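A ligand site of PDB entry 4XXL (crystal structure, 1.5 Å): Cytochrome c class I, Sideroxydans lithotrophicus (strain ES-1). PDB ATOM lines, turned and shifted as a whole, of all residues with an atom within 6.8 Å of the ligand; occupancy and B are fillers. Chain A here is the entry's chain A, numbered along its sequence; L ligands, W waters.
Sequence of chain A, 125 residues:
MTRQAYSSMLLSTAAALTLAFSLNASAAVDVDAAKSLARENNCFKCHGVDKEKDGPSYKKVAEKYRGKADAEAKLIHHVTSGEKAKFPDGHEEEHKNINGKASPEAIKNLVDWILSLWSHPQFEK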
ATOM      1  N   LEU A  37      27.199  35.651  -6.346  1.00  0.00           N
ATOM      2  CA  LEU A  37      27.745  35.098  -5.114  1.00  0.00           C
ATOM      3  C   LEU A  37      27.643  33.554  -5.080  1.00  0.00           C
ATOM      4  O   LEU A  37      28.574  32.833  -4.647  1.00  0.00           O
ATOM      5  CB  LEU A  37      27.057  35.735  -3.901  1.00  0.00           C
ATOM      6  CG  LEU A  37      27.770  35.457  -2.573  1.00  0.00           C
ATOM      7  CD1 LEU A  37      29.140  36.114  -2.516  1.00  0.00           C
ATOM      8  CD2 LEU A  37      26.924  35.917  -1.427  1.00  0.00           C
ATOM      9  N   ALA A  38      26.499  33.048  -5.557  1.00  0.00           N
ATOM     10  CA  ALA A  38      26.297  31.576  -5.646  1.00  0.00           C
ATOM     11  C   ALA A  38      27.342  30.948  -6.592  1.00  0.00           C
ATOM     12  O   ALA A  38      27.936  29.925  -6.254  1.00  0.00           O
ATOM     13  CB  ALA A  38      24.882  31.230  -6.106  1.00  0.00           C
ATOM     14  N   ASN A  41      30.937  30.832  -5.027  1.00  0.00           N
ATOM     15  CA  ASN A  41      31.138  29.979  -3.867  1.00  0.00           C
ATOM     16  C   ASN A  41      30.677  28.549  -4.032  1.00  0.00           C
ATOM     17  O   ASN A  41      30.481  27.804  -3.103  1.00  0.00           O
ATOM     18  CB  ASN A  41      30.509  30.661  -2.669  1.00  0.00           C
ATOM     19  CG  ASN A  41      31.268  31.888  -2.245  1.00  0.00           C
ATOM     20  OD1 ASN A  41      32.310  31.779  -1.601  1.00  0.00           O
ATOM     21  ND2 ASN A  41      30.761  33.060  -2.609  1.00  0.00           N
ATOM     22  N   ASN A  42      30.536  28.141  -5.283  1.00  0.00           N
ATOM     23  CA  ASN A  42      30.309  26.765  -5.720  1.00  0.00           C
ATOM     24  C   ASN A  42      28.904  26.258  -5.452  1.00  0.00           C
ATOM     25  O   ASN A  42      28.638  25.056  -5.483  1.00  0.00           O
ATOM     26  CB  ASN A  42      31.379  25.807  -5.117  1.00  0.00           C
ATOM     27  CG  ASN A  42      32.654  25.777  -5.913  1.00  0.00           C
ATOM     28  OD1 ASN A  42      32.703  26.211  -7.052  1.00  0.00           O
ATOM     29  ND2 ASN A  42      33.682  25.140  -5.341  1.00  0.00           N
ATOM     30  N   CYS A  43      28.027  27.168  -5.065  1.00  0.00           N
ATOM     31  CA  CYS A  43      26.694  26.768  -4.674  1.00  0.00           C
ATOM     32  C   CYS A  43      25.983  26.012  -5.775  1.00  0.00           C
ATOM     33  O   CYS A  43      25.332  24.993  -5.460  1.00  0.00           O
ATOM     34  CB  CYS A  43      25.912  28.028  -4.231  1.00  0.00           C
ATOM     35  SG  CYS A  43      26.653  29.027  -2.982  1.00  0.00           S
ATOM     36  N   PHE A  44      26.105  26.458  -6.996  1.00  0.00           N
ATOM     37  CA  PHE A  44      25.403  25.845  -8.134  1.00  0.00           C
ATOM     38  C   PHE A  44      26.079  24.526  -8.555  1.00  0.00           C
ATOM     39  O   PHE A  44      25.533  23.769  -9.333  1.00  0.00           O
ATOM     40  CB  PHE A  44      25.323  26.791  -9.293  1.00  0.00           C
ATOM     41  CG  PHE A  44      24.383  27.943  -9.086  1.00  0.00           C
ATOM     42  CD1 PHE A  44      23.147  27.810  -8.508  1.00  0.00           C
ATOM     43  CD2 PHE A  44      24.768  29.216  -9.510  1.00  0.00           C
ATOM     44  CE1 PHE A  44      22.278  28.917  -8.401  1.00  0.00           C
ATOM     45  CE2 PHE A  44      23.934  30.304  -9.415  1.00  0.00           C
ATOM     46  CZ  PHE A  44      22.685  30.167  -8.832  1.00  0.00           C
ATOM     47  N   LYS A  45      27.232  24.191  -7.991  1.00  0.00           N
ATOM     48  CA  LYS A  45      27.791  22.853  -8.303  1.00  0.00           C
ATOM     49  C   LYS A  45      26.930  21.753  -7.687  1.00  0.00           C
ATOM     50  O   LYS A  45      26.885  20.645  -8.200  1.00  0.00           O
ATOM     51  CB  LYS A  45      29.230  22.746  -7.801  1.00  0.00           C
ATOM     52  CG  LYS A  45      30.170  23.761  -8.374  1.00  0.00           C
ATOM     53  CD  LYS A  45      30.189  23.693  -9.901  1.00  0.00           C
ATOM     54  CE  LYS A  45      31.428  24.292 -10.524  1.00  0.00           C
ATOM     55  NZ  LYS A  45      31.852  25.557  -9.914  1.00  0.00           N
ATOM     56  N   CYS A  46      26.273  22.073  -6.592  1.00  0.00           N
ATOM     57  CA  CYS A  46      25.433  21.101  -5.929  1.00  0.00           C
ATOM     58  C   CYS A  46      23.923  21.396  -5.955  1.00  0.00           C
ATOM     59  O   CYS A  46      23.142  20.534  -5.590  1.00  0.00           O
ATOM     60  CB  CYS A  46      25.886  20.996  -4.513  1.00  0.00           C
ATOM     61  SG  CYS A  46      27.548  20.268  -4.295  1.00  0.00           S
ATOM     62  N   HIS A  47      23.542  22.653  -6.223  1.00  0.00           N
ATOM     63  CA  HIS A  47      22.139  23.095  -6.142  1.00  0.00           C
ATOM     64  C   HIS A  47      21.715  23.651  -7.466  1.00  0.00           C
ATOM     65  O   HIS A  47      22.499  24.379  -8.086  1.00  0.00           O
ATOM     66  CB  HIS A  47      21.947  24.158  -5.052  1.00  0.00           C
ATOM     67  CG  HIS A  47      22.225  23.678  -3.636  1.00  0.00           C
ATOM     68  ND1 HIS A  47      21.272  23.015  -2.899  1.00  0.00           N
ATOM     69  CD2 HIS A  47      23.297  23.837  -2.822  1.00  0.00           C
ATOM     70  CE1 HIS A  47      21.744  22.833  -1.667  1.00  0.00           C
ATOM     71  NE2 HIS A  47      23.008  23.267  -1.622  1.00  0.00           N
ATOM     72  N   ASP A  54      23.228  17.213  -6.012  1.00  0.00           N
ATOM     73  CA  ASP A  54      23.759  16.666  -4.734  1.00  0.00           C
ATOM     74  C   ASP A  54      22.938  17.239  -3.546  1.00  0.00           C
ATOM     75  O   ASP A  54      22.535  16.534  -2.581  1.00  0.00           O
ATOM     76  CB  ASP A  54      25.253  17.004  -4.577  1.00  0.00           C
ATOM     77  CG  ASP A  54      26.104  16.728  -5.860  1.00  0.00           C
ATOM     78  OD1 ASP A  54      25.993  17.504  -6.870  1.00  0.00           O
ATOM     79  OD2 ASP A  54      26.945  15.791  -5.790  1.00  0.00           O
ATOM     80  N   GLY A  55      22.600  18.523  -3.679  1.00  0.00           N
ATOM     81  CA  GLY A  55      21.805  19.243  -2.719  1.00  0.00           C
ATOM     82  C   GLY A  55      20.384  19.515  -3.236  1.00  0.00           C
ATOM     83  O   GLY A  55      20.087  19.298  -4.412  1.00  0.00           O
ATOM     84  N   PRO A  56      19.438  19.858  -2.373  1.00  0.00           N
ATOM     85  CA  PRO A  56      18.028  20.134  -2.793  1.00  0.00           C
ATOM     86  C   PRO A  56      17.943  21.329  -3.728  1.00  0.00           C
ATOM     87  O   PRO A  56      18.805  22.255  -3.665  1.00  0.00           O
ATOM     88  CB  PRO A  56      17.307  20.438  -1.490  1.00  0.00           C
ATOM     89  CG  PRO A  56      18.418  20.911  -0.610  1.00  0.00           C
ATOM     90  CD  PRO A  56      19.608  20.076  -0.934  1.00  0.00           C
ATOM     91  N   TYR A  58      16.679  24.883  -5.002  1.00  0.00           N
ATOM     92  CA  TYR A  58      16.371  26.008  -4.162  1.00  0.00           C
ATOM     93  C   TYR A  58      14.879  26.252  -4.122  1.00  0.00           C
ATOM     94  O   TYR A  58      14.406  26.803  -3.165  1.00  0.00           O
ATOM     95  CB  TYR A  58      17.126  27.262  -4.573  1.00  0.00           C
ATOM     96  CG  TYR A  58      18.612  27.178  -4.255  1.00  0.00           C
ATOM     97  CD1 TYR A  58      19.074  26.537  -3.118  1.00  0.00           C
ATOM     98  CD2 TYR A  58      19.556  27.829  -5.041  1.00  0.00           C
ATOM     99  CE1 TYR A  58      20.443  26.541  -2.800  1.00  0.00           C
ATOM    100  CE2 TYR A  58      20.902  27.831  -4.739  1.00  0.00           C
ATOM    101  CZ  TYR A  58      21.355  27.198  -3.615  1.00  0.00           C
ATOM    102  OH  TYR A  58      22.687  27.219  -3.307  1.00  0.00           O
ATOM    103  N   VAL A  61      13.816  24.160  -1.255  1.00  0.00           N
ATOM    104  CA  VAL A  61      14.177  24.839  -0.011  1.00  0.00           C
ATOM    105  C   VAL A  61      13.194  25.943   0.276  1.00  0.00           C
ATOM    106  O   VAL A  61      12.775  26.171   1.432  1.00  0.00           O
ATOM    107  CB  VAL A  61      15.595  25.453  -0.106  1.00  0.00           C
ATOM    108  CG1 VAL A  61      15.909  26.264   1.132  1.00  0.00           C
ATOM    109  CG2 VAL A  61      16.611  24.282  -0.198  1.00  0.00           C
ATOM    110  N   LYS A  64      10.115  24.551   1.627  1.00  0.00           N
ATOM    111  CA  LYS A  64      10.271  24.101   2.981  1.00  0.00           C
ATOM    112  C   LYS A  64      10.191  25.224   3.990  1.00  0.00           C
ATOM    113  O   LYS A  64       9.582  25.092   5.017  1.00  0.00           O
ATOM    114  CB  LYS A  64      11.637  23.433   3.112  1.00  0.00           C
ATOM    115  CG  LYS A  64      12.078  23.267   4.538  1.00  0.00           C
ATOM    116  CD  LYS A  64      13.355  22.397   4.642  1.00  0.00           C
ATOM    117  CE  LYS A  64      13.923  22.458   6.038  1.00  0.00           C
ATOM    118  NZ  LYS A  64      15.278  21.867   6.192  1.00  0.00           N
ATOM    119  N   TYR A  65      10.707  26.382   3.609  1.00  0.00           N
ATOM    120  CA  TYR A  65      10.769  27.463   4.565  1.00  0.00           C
ATOM    121  C   TYR A  65       9.658  28.502   4.392  1.00  0.00           C
ATOM    122  O   TYR A  65       9.597  29.441   5.176  1.00  0.00           O
ATOM    123  CB  TYR A  65      12.128  28.213   4.444  1.00  0.00           C
ATOM    124  CG  TYR A  65      13.200  27.456   5.188  1.00  0.00           C
ATOM    125  CD1 TYR A  65      13.373  27.674   6.545  1.00  0.00           C
ATOM    126  CD2 TYR A  65      13.992  26.483   4.580  1.00  0.00           C
ATOM    127  CE1 TYR A  65      14.314  26.942   7.278  1.00  0.00           C
ATOM    128  CE2 TYR A  65      14.933  25.755   5.299  1.00  0.00           C
ATOM    129  CZ  TYR A  65      15.091  25.988   6.653  1.00  0.00           C
ATOM    130  OH  TYR A  65      16.035  25.268   7.367  1.00  0.00           O
ATOM    131  N   LYS A  74      17.588  31.516   9.863  1.00  0.00           N
ATOM    132  CA  LYS A  74      17.958  30.098   9.824  1.00  0.00           C
ATOM    133  C   LYS A  74      18.882  29.761   8.666  1.00  0.00           C
ATOM    134  O   LYS A  74      19.795  28.932   8.859  1.00  0.00           O
ATOM    135  CB  LYS A  74      16.766  29.157   9.731  1.00  0.00           C
ATOM    136  CG  LYS A  74      15.985  28.995  11.025  1.00  0.00           C
ATOM    137  CD  LYS A  74      16.375  27.736  11.795  1.00  0.00           C
ATOM    138  CE  LYS A  74      15.142  27.003  12.332  1.00  0.00           C
ATOM    139  NZ  LYS A  74      14.681  27.506  13.652  1.00  0.00           N
ATOM    140  N   LEU A  75      18.604  30.327   7.505  1.00  0.00           N
ATOM    141  CA  LEU A  75      19.463  30.018   6.338  1.00  0.00           C
ATOM    142  C   LEU A  75      20.770  30.790   6.391  1.00  0.00           C
ATOM    143  O   LEU A  75      21.814  30.274   5.951  1.00  0.00           O
ATOM    144  CB  LEU A  75      18.755  30.256   4.983  1.00  0.00           C
ATOM    145  CG  LEU A  75      17.610  29.280   4.586  1.00  0.00           C
ATOM    146  CD1 LEU A  75      17.221  29.446   3.146  1.00  0.00           C
ATOM    147  CD2 LEU A  75      18.019  27.816   4.845  1.00  0.00           C
ATOM    148  N   HIS A  78      22.665  28.571   8.495  1.00  0.00           N
ATOM    149  CA  HIS A  78      23.034  27.352   7.799  1.00  0.00           C
ATOM    150  C   HIS A  78      24.256  27.545   6.898  1.00  0.00           C
ATOM    151  O   HIS A  78      25.088  26.648   6.802  1.00  0.00           O
ATOM    152  CB  HIS A  78      21.884  26.890   6.913  1.00  0.00           C
ATOM    153  CG  HIS A  78      22.240  25.731   6.043  1.00  0.00           C
ATOM    154  ND1 HIS A  78      22.604  25.847   4.723  1.00  0.00           N
ATOM    155  CD2 HIS A  78      22.332  24.412   6.350  1.00  0.00           C
ATOM    156  CE1 HIS A  78      22.894  24.653   4.253  1.00  0.00           C
ATOM    157  NE2 HIS A  78      22.690  23.768   5.207  1.00  0.00           N
ATOM    158  N   VAL A  79      24.346  28.665   6.204  1.00  0.00           N
ATOM    159  CA  VAL A  79      25.470  28.888   5.281  1.00  0.00           C
ATOM    160  C   VAL A  79      26.766  29.427   5.884  1.00  0.00           C
ATOM    161  O   VAL A  79      27.800  29.564   5.175  1.00  0.00           O
ATOM    162  CB  VAL A  79      24.969  29.739   4.132  1.00  0.00           C
ATOM    163  CG1 VAL A  79      24.874  31.223   4.466  1.00  0.00           C
ATOM    164  CG2 VAL A  79      25.754  29.459   2.846  1.00  0.00           C
ATOM    165  N   LYS A  84      26.591  19.604   9.765  1.00  0.00           N
ATOM    166  CA  LYS A  84      26.476  18.409   8.935  1.00  0.00           C
ATOM    167  C   LYS A  84      25.416  18.540   7.840  1.00  0.00           C
ATOM    168  O   LYS A  84      24.321  19.127   7.997  1.00  0.00           O
ATOM    169  CB  LYS A  84      26.257  17.143   9.780  1.00  0.00           C
ATOM    170  CG  LYS A  84      27.492  16.816  10.638  1.00  0.00           C
ATOM    171  CD  LYS A  84      28.593  16.073   9.858  1.00  0.00           C
ATOM    172  CE  LYS A  84      28.455  14.548  10.007  1.00  0.00           C
ATOM    173  NZ  LYS A  84      29.648  13.742   9.587  1.00  0.00           N
ATOM    174  N   ALA A  85      25.768  17.994   6.696  1.00  0.00           N
ATOM    175  CA  ALA A  85      24.907  17.989   5.522  1.00  0.00           C
ATOM    176  C   ALA A  85      24.880  16.543   5.100  1.00  0.00           C
ATOM    177  O   ALA A  85      25.934  15.901   4.969  1.00  0.00           O
ATOM    178  CB  ALA A  85      25.450  18.898   4.410  1.00  0.00           C
ATOM    179  N   LYS A  86      23.649  16.001   5.030  1.00  0.00           N
ATOM    180  CA  LYS A  86      23.483  14.604   4.655  1.00  0.00           C
ATOM    181  C   LYS A  86      23.243  14.549   3.168  1.00  0.00           C
ATOM    182  O   LYS A  86      22.349  15.199   2.611  1.00  0.00           O
ATOM    183  CB  LYS A  86      22.330  13.973   5.418  1.00  0.00           C
ATOM    184  CG  LYS A  86      21.913  12.631   4.867  1.00  0.00           C
ATOM    185  CD  LYS A  86      22.996  11.603   5.042  1.00  0.00           C
ATOM    186  CE  LYS A  86      22.437  10.353   5.719  1.00  0.00           C
ATOM    187  NZ  LYS A  86      22.280  10.609   7.180  1.00  0.00           N
ATOM    188  N   PHE A  87      24.068  13.737   2.484  1.00  0.00           N
ATOM    189  CA  PHE A  87      23.988  13.618   1.019  1.00  0.00           C
ATOM    190  C   PHE A  87      23.044  12.499   0.592  1.00  0.00           C
ATOM    191  O   PHE A  87      22.774  11.532   1.385  1.00  0.00           O
ATOM    192  CB  PHE A  87      25.378  13.461   0.381  1.00  0.00           C
ATOM    193  CG  PHE A  87      26.193  14.740   0.342  1.00  0.00           C
ATOM    194  CD1 PHE A  87      26.596  15.347   1.506  1.00  0.00           C
ATOM    195  CD2 PHE A  87      26.520  15.353  -0.867  1.00  0.00           C
ATOM    196  CE1 PHE A  87      27.337  16.515   1.460  1.00  0.00           C
ATOM    197  CE2 PHE A  87      27.278  16.534  -0.900  1.00  0.00           C
ATOM    198  CZ  PHE A  87      27.627  17.118   0.255  1.00  0.00           C
ATOM    199  N   PRO A  88      22.620  12.512  -0.696  1.00  0.00           N
ATOM    200  CA  PRO A  88      21.698  11.512  -1.153  1.00  0.00           C
ATOM    201  C   PRO A  88      22.194  10.073  -0.987  1.00  0.00           C
ATOM    202  O   PRO A  88      21.380   9.200  -0.597  1.00  0.00           O
ATOM    203  CB  PRO A  88      21.535  11.887  -2.641  1.00  0.00           C
ATOM    204  CG  PRO A  88      21.553  13.373  -2.635  1.00  0.00           C
ATOM    205  CD  PRO A  88      22.713  13.623  -1.695  1.00  0.00           C
ATOM    206  N   GLU A  93      28.931  15.403   5.085  1.00  0.00           N
ATOM    207  CA  GLU A  93      30.063  16.365   5.012  1.00  0.00           C
ATOM    208  C   GLU A  93      29.628  17.584   5.817  1.00  0.00           C
ATOM    209  O   GLU A  93      28.459  17.798   6.014  1.00  0.00           O
ATOM    210  CB  GLU A  93      30.338  16.860   3.589  1.00  0.00           C
ATOM    211  CG  GLU A  93      30.634  15.738   2.602  1.00  0.00           C
ATOM    212  CD  GLU A  93      30.948  16.223   1.185  1.00  0.00           C
ATOM    213  OE1 GLU A  93      31.106  17.455   0.933  1.00  0.00           O
ATOM    214  OE2 GLU A  93      31.013  15.321   0.279  1.00  0.00           O
ATOM    215  N   HIS A  95      28.696  21.300   5.748  1.00  0.00           N
ATOM    216  CA  HIS A  95      28.220  22.128   4.615  1.00  0.00           C
ATOM    217  C   HIS A  95      29.205  23.261   4.316  1.00  0.00           C
ATOM    218  O   HIS A  95      29.842  23.766   5.272  1.00  0.00           O
ATOM    219  CB  HIS A  95      26.817  22.647   4.853  1.00  0.00           C
ATOM    220  CG  HIS A  95      26.136  23.267   3.636  1.00  0.00           C
ATOM    221  ND1 HIS A  95      26.382  24.561   3.251  1.00  0.00           N
ATOM    222  CD2 HIS A  95      25.408  22.731   2.616  1.00  0.00           C
ATOM    223  CE1 HIS A  95      25.745  24.823   2.127  1.00  0.00           C
ATOM    224  NE2 HIS A  95      25.059  23.755   1.732  1.00  0.00           N
ATOM    225  N   LYS A  96      29.307  23.636   3.043  1.00  0.00           N
ATOM    226  CA  LYS A  96      30.042  24.851   2.576  1.00  0.00           C
ATOM    227  C   LYS A  96      29.748  26.010   3.544  1.00  0.00           C
ATOM    228  O   LYS A  96      28.582  26.253   3.898  1.00  0.00           O
ATOM    229  CB  LYS A  96      29.601  25.211   1.171  1.00  0.00           C
ATOM    230  CG  LYS A  96      30.250  26.470   0.625  1.00  0.00           C
ATOM    231  CD  LYS A  96      31.699  26.240   0.395  1.00  0.00           C
ATOM    232  CE  LYS A  96      32.327  27.428  -0.327  1.00  0.00           C
ATOM    233  NZ  LYS A  96      33.773  27.198  -0.476  1.00  0.00           N
ATOM    234  N   ASN A  97      30.799  26.633   4.047  1.00  0.00           N
ATOM    235  CA  ASN A  97      30.668  27.712   5.033  1.00  0.00           C
ATOM    236  C   ASN A  97      31.243  28.963   4.409  1.00  0.00           C
ATOM    237  O   ASN A  97      32.464  29.005   4.187  1.00  0.00           O
ATOM    238  CB  ASN A  97      31.406  27.316   6.297  1.00  0.00           C
ATOM    239  CG  ASN A  97      31.309  28.327   7.353  1.00  0.00           C
ATOM    240  OD1 ASN A  97      30.894  29.456   7.133  1.00  0.00           O
ATOM    241  ND2 ASN A  97      31.697  27.940   8.512  1.00  0.00           N
ATOM    242  N   ILE A  98      30.410  29.960   4.159  1.00  0.00           N
ATOM    243  CA  ILE A  98      30.905  31.190   3.577  1.00  0.00           C
ATOM    244  C   ILE A  98      31.120  32.317   4.619  1.00  0.00           C
ATOM    245  O   ILE A  98      31.310  33.522   4.235  1.00  0.00           O
ATOM    246  CB  ILE A  98      30.063  31.665   2.371  1.00  0.00           C
ATOM    247  CG1 ILE A  98      28.631  31.901   2.788  1.00  0.00           C
ATOM    248  CG2 ILE A  98      30.211  30.636   1.231  1.00  0.00           C
ATOM    249  CD1 ILE A  98      27.780  32.474   1.663  1.00  0.00           C
ATOM    250  N   LEU A 110      21.672  36.874  -0.819  1.00  0.00           N
ATOM    251  CA  LEU A 110      21.596  35.535  -1.417  1.00  0.00           C
ATOM    252  C   LEU A 110      20.508  34.643  -0.738  1.00  0.00           C
ATOM    253  O   LEU A 110      19.718  34.014  -1.434  1.00  0.00           O
ATOM    254  CB  LEU A 110      22.916  34.807  -1.314  1.00  0.00           C
ATOM    255  CG  LEU A 110      22.934  33.331  -1.699  1.00  0.00           C
ATOM    256  CD1 LEU A 110      22.445  33.058  -3.105  1.00  0.00           C
ATOM    257  CD2 LEU A 110      24.350  32.825  -1.592  1.00  0.00           C
ATOM    258  N   VAL A 111      20.429  34.658   0.579  1.00  0.00           N
ATOM    259  CA  VAL A 111      19.390  33.961   1.333  1.00  0.00           C
ATOM    260  C   VAL A 111      18.032  34.436   0.894  1.00  0.00           C
ATOM    261  O   VAL A 111      17.106  33.657   0.673  1.00  0.00           O
ATOM    262  CB  VAL A 111      19.642  34.094   2.859  1.00  0.00           C
ATOM    263  CG1 VAL A 111      18.424  33.615   3.703  1.00  0.00           C
ATOM    264  CG2 VAL A 111      20.863  33.221   3.219  1.00  0.00           C
ATOM    265  N   ILE A 114      17.134  32.981  -2.493  1.00  0.00           N
ATOM    266  CA  ILE A 114      16.719  31.599  -2.317  1.00  0.00           C
ATOM    267  C   ILE A 114      15.297  31.443  -1.804  1.00  0.00           C
ATOM    268  O   ILE A 114      14.516  30.644  -2.373  1.00  0.00           O
ATOM    269  CB  ILE A 114      17.737  30.810  -1.429  1.00  0.00           C
ATOM    270  CG1 ILE A 114      19.072  30.625  -2.210  1.00  0.00           C
ATOM    271  CG2 ILE A 114      17.158  29.469  -0.965  1.00  0.00           C
ATOM    272  CD1 ILE A 114      20.235  30.164  -1.337  1.00  0.00           C
HETATM  273 FE1  LIG L   1      24.023  23.478   0.085  1.00  0.00          FE
HETATM  274  C1  LIG L   1      21.422  22.079   1.930  1.00  0.00           C
HETATM  275  C2  LIG L   1      22.518  26.584   0.294  1.00  0.00           C
HETATM  276  C3  LIG L   1      26.834  24.932  -1.293  1.00  0.00           C
HETATM  277  C4  LIG L   1      25.188  20.416  -0.683  1.00  0.00           C
HETATM  278  N1  LIG L   1      22.316  24.178   1.003  1.00  0.00           N
HETATM  279  C5  LIG L   1      21.373  23.429   1.619  1.00  0.00           C
HETATM  280  C6  LIG L   1      20.293  24.298   1.942  1.00  0.00           C
HETATM  281  C7  LIG L   1      20.619  25.543   1.456  1.00  0.00           C
HETATM  282  C8  LIG L   1      21.903  25.466   0.853  1.00  0.00           C
HETATM  283  C9  LIG L   1      19.800  26.796   1.490  1.00  0.00           C
HETATM  284  C10 LIG L   1      19.041  23.834   2.686  1.00  0.00           C
HETATM  285  C11 LIG L   1      19.285  23.926   4.177  1.00  0.00           C
HETATM  286  C12 LIG L   1      18.057  23.618   5.021  1.00  0.00           C
HETATM  287  O1  LIG L   1      17.092  23.025   4.515  1.00  0.00           O
HETATM  288  O2  LIG L   1      18.001  24.088   6.202  1.00  0.00           O
HETATM  289  N2  LIG L   1      24.579  25.358  -0.416  1.00  0.00           N
HETATM  290  C13 LIG L   1      23.814  26.495  -0.238  1.00  0.00           C
HETATM  291  C14 LIG L   1      24.552  27.633  -0.691  1.00  0.00           C
HETATM  292  C15 LIG L   1      25.756  27.225  -1.123  1.00  0.00           C
HETATM  293  C16 LIG L   1      25.802  25.780  -0.937  1.00  0.00           C
HETATM  294  C17 LIG L   1      24.041  29.043  -0.644  1.00  0.00           C
HETATM  295  C18 LIG L   1      26.930  28.012  -1.580  1.00  0.00           C
HETATM  296  C19 LIG L   1      27.386  28.843  -0.539  1.00  0.00           C
HETATM  297  N3  LIG L   1      25.719  22.757  -0.876  1.00  0.00           N
HETATM  298  C20 LIG L   1      26.714  23.575  -1.299  1.00  0.00           C
HETATM  299  C21 LIG L   1      27.617  22.702  -1.940  1.00  0.00           C
HETATM  300  C22 LIG L   1      27.168  21.396  -1.883  1.00  0.00           C
HETATM  301  C23 LIG L   1      25.953  21.482  -1.142  1.00  0.00           C
HETATM  302  C24 LIG L   1      28.823  23.205  -2.644  1.00  0.00           C
HETATM  303  C25 LIG L   1      27.818  20.165  -2.500  1.00  0.00           C
HETATM  304  C26 LIG L   1      29.150  19.876  -2.189  1.00  0.00           C
HETATM  305  N4  LIG L   1      23.466  21.680   0.582  1.00  0.00           N
HETATM  306  C27 LIG L   1      24.044  20.502   0.142  1.00  0.00           C
HETATM  307  C28 LIG L   1      23.363  19.319   0.716  1.00  0.00           C
HETATM  308  C29 LIG L   1      22.352  19.809   1.423  1.00  0.00           C
HETATM  309  C30 LIG L   1      22.374  21.274   1.311  1.00  0.00           C
HETATM  310  C31 LIG L   1      23.741  17.909   0.488  1.00  0.00           C
HETATM  311  C32 LIG L   1      21.282  19.004   2.180  1.00  0.00           C
HETATM  312  C33 LIG L   1      21.701  18.754   3.596  1.00  0.00           C
HETATM  313  C34 LIG L   1      20.717  17.954   4.454  1.00  0.00           C
HETATM  314  O3  LIG L   1      19.478  17.860   4.179  1.00  0.00           O
HETATM  315  O4  LIG L   1      21.163  17.430   5.515  1.00  0.00           O
HETATM  316  O   HOH W   1      20.156  21.505   7.029  1.00  0.00           O
HETATM  317  O   HOH W   2      28.385  21.586   1.198  1.00  0.00           O
HETATM  318  O   HOH W   3      19.549  24.327   8.371  1.00  0.00           O
HETATM  319  O   HOH W   4      18.020  20.499   3.081  1.00  0.00           O
HETATM  320  O   HOH W   5      22.756  21.007   5.078  1.00  0.00           O
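Merely in contact with the ligand: Tyr 58, His 78, Asn 42, Asp 54, Pro 56, Lys 96, Gly 55, Ile 98, Ala 85, Val 61, Val 79, Asn 41, Leu 110, Leu 75 and Phe 87. Hydrophobic or aromatic side chains within 4 Å of the ligand: His 47, Pro 56, Tyr 58, Val 61, Tyr 65, Leu 75, His 78, Val 79, Ala 85, Phe 87, His 95, Ile 98 and Leu 110. The nearest printed residue that does not touch the ligand is Ile 114 (4.03 Å).
The backbone carbonyl oxygen of Ala 38 lies within hydrogen-bond range of the backbone NH of Cys 43 (3.0 Å). A ring nitrogen (ND1) of His 47 is in hydrogen-bond range of the backbone carbonyl oxygen (O) of Pro 56 (2.7 Å). The backbone NH (N) of Gly 55 sits at hydrogen-bond distance from the backbone carbonyl oxygen (O) of Cys 46, 2.8 Å away. The backbone carbonyl oxygen (O) of Glu 93 is in hydrogen-bond range of the backbone NH (N) of Ala 85, 2.8 Å away. The side-chain amide oxygen (OD1) of Asn 42 lies within hydrogen-bond range of the side-chain amino group (NZ) of Lys 45. The backbone carbonyl oxygen of Cys 46 is in hydrogen-bond range of the backbone NH of Asp 54, 3.3 Å away. ND2 of Asn 41 is in hydrogen-bond range of O of Leu 37. The backbone NH (N) of Ile 98 sits at hydrogen-bond distance from the backbone carbonyl oxygen (O) of Val 79, at 2.8 Å.
SG of Cys 43 is covalently linked to C18 of the ligand. The backbone NH (N) of Lys 86 lies within hydrogen-bond range of an oxygen (O4) of the ligand (2.9 Å). NZ of Lys 64 is in salt-bridge range of O1 of the ligand (2.7 Å). A ring nitrogen (NE2) of His 95 binds an iron atom (FE1) of the ligand (2.0 Å). C25 of the ligand is covalently linked to SG of Cys 46 (1.8 Å). A ring nitrogen (NE2) of His 47 binds an iron atom (FE1) of the ligand. OH of Tyr 65 sits at hydrogen-bond distance from O2 of the ligand (2.6 Å).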
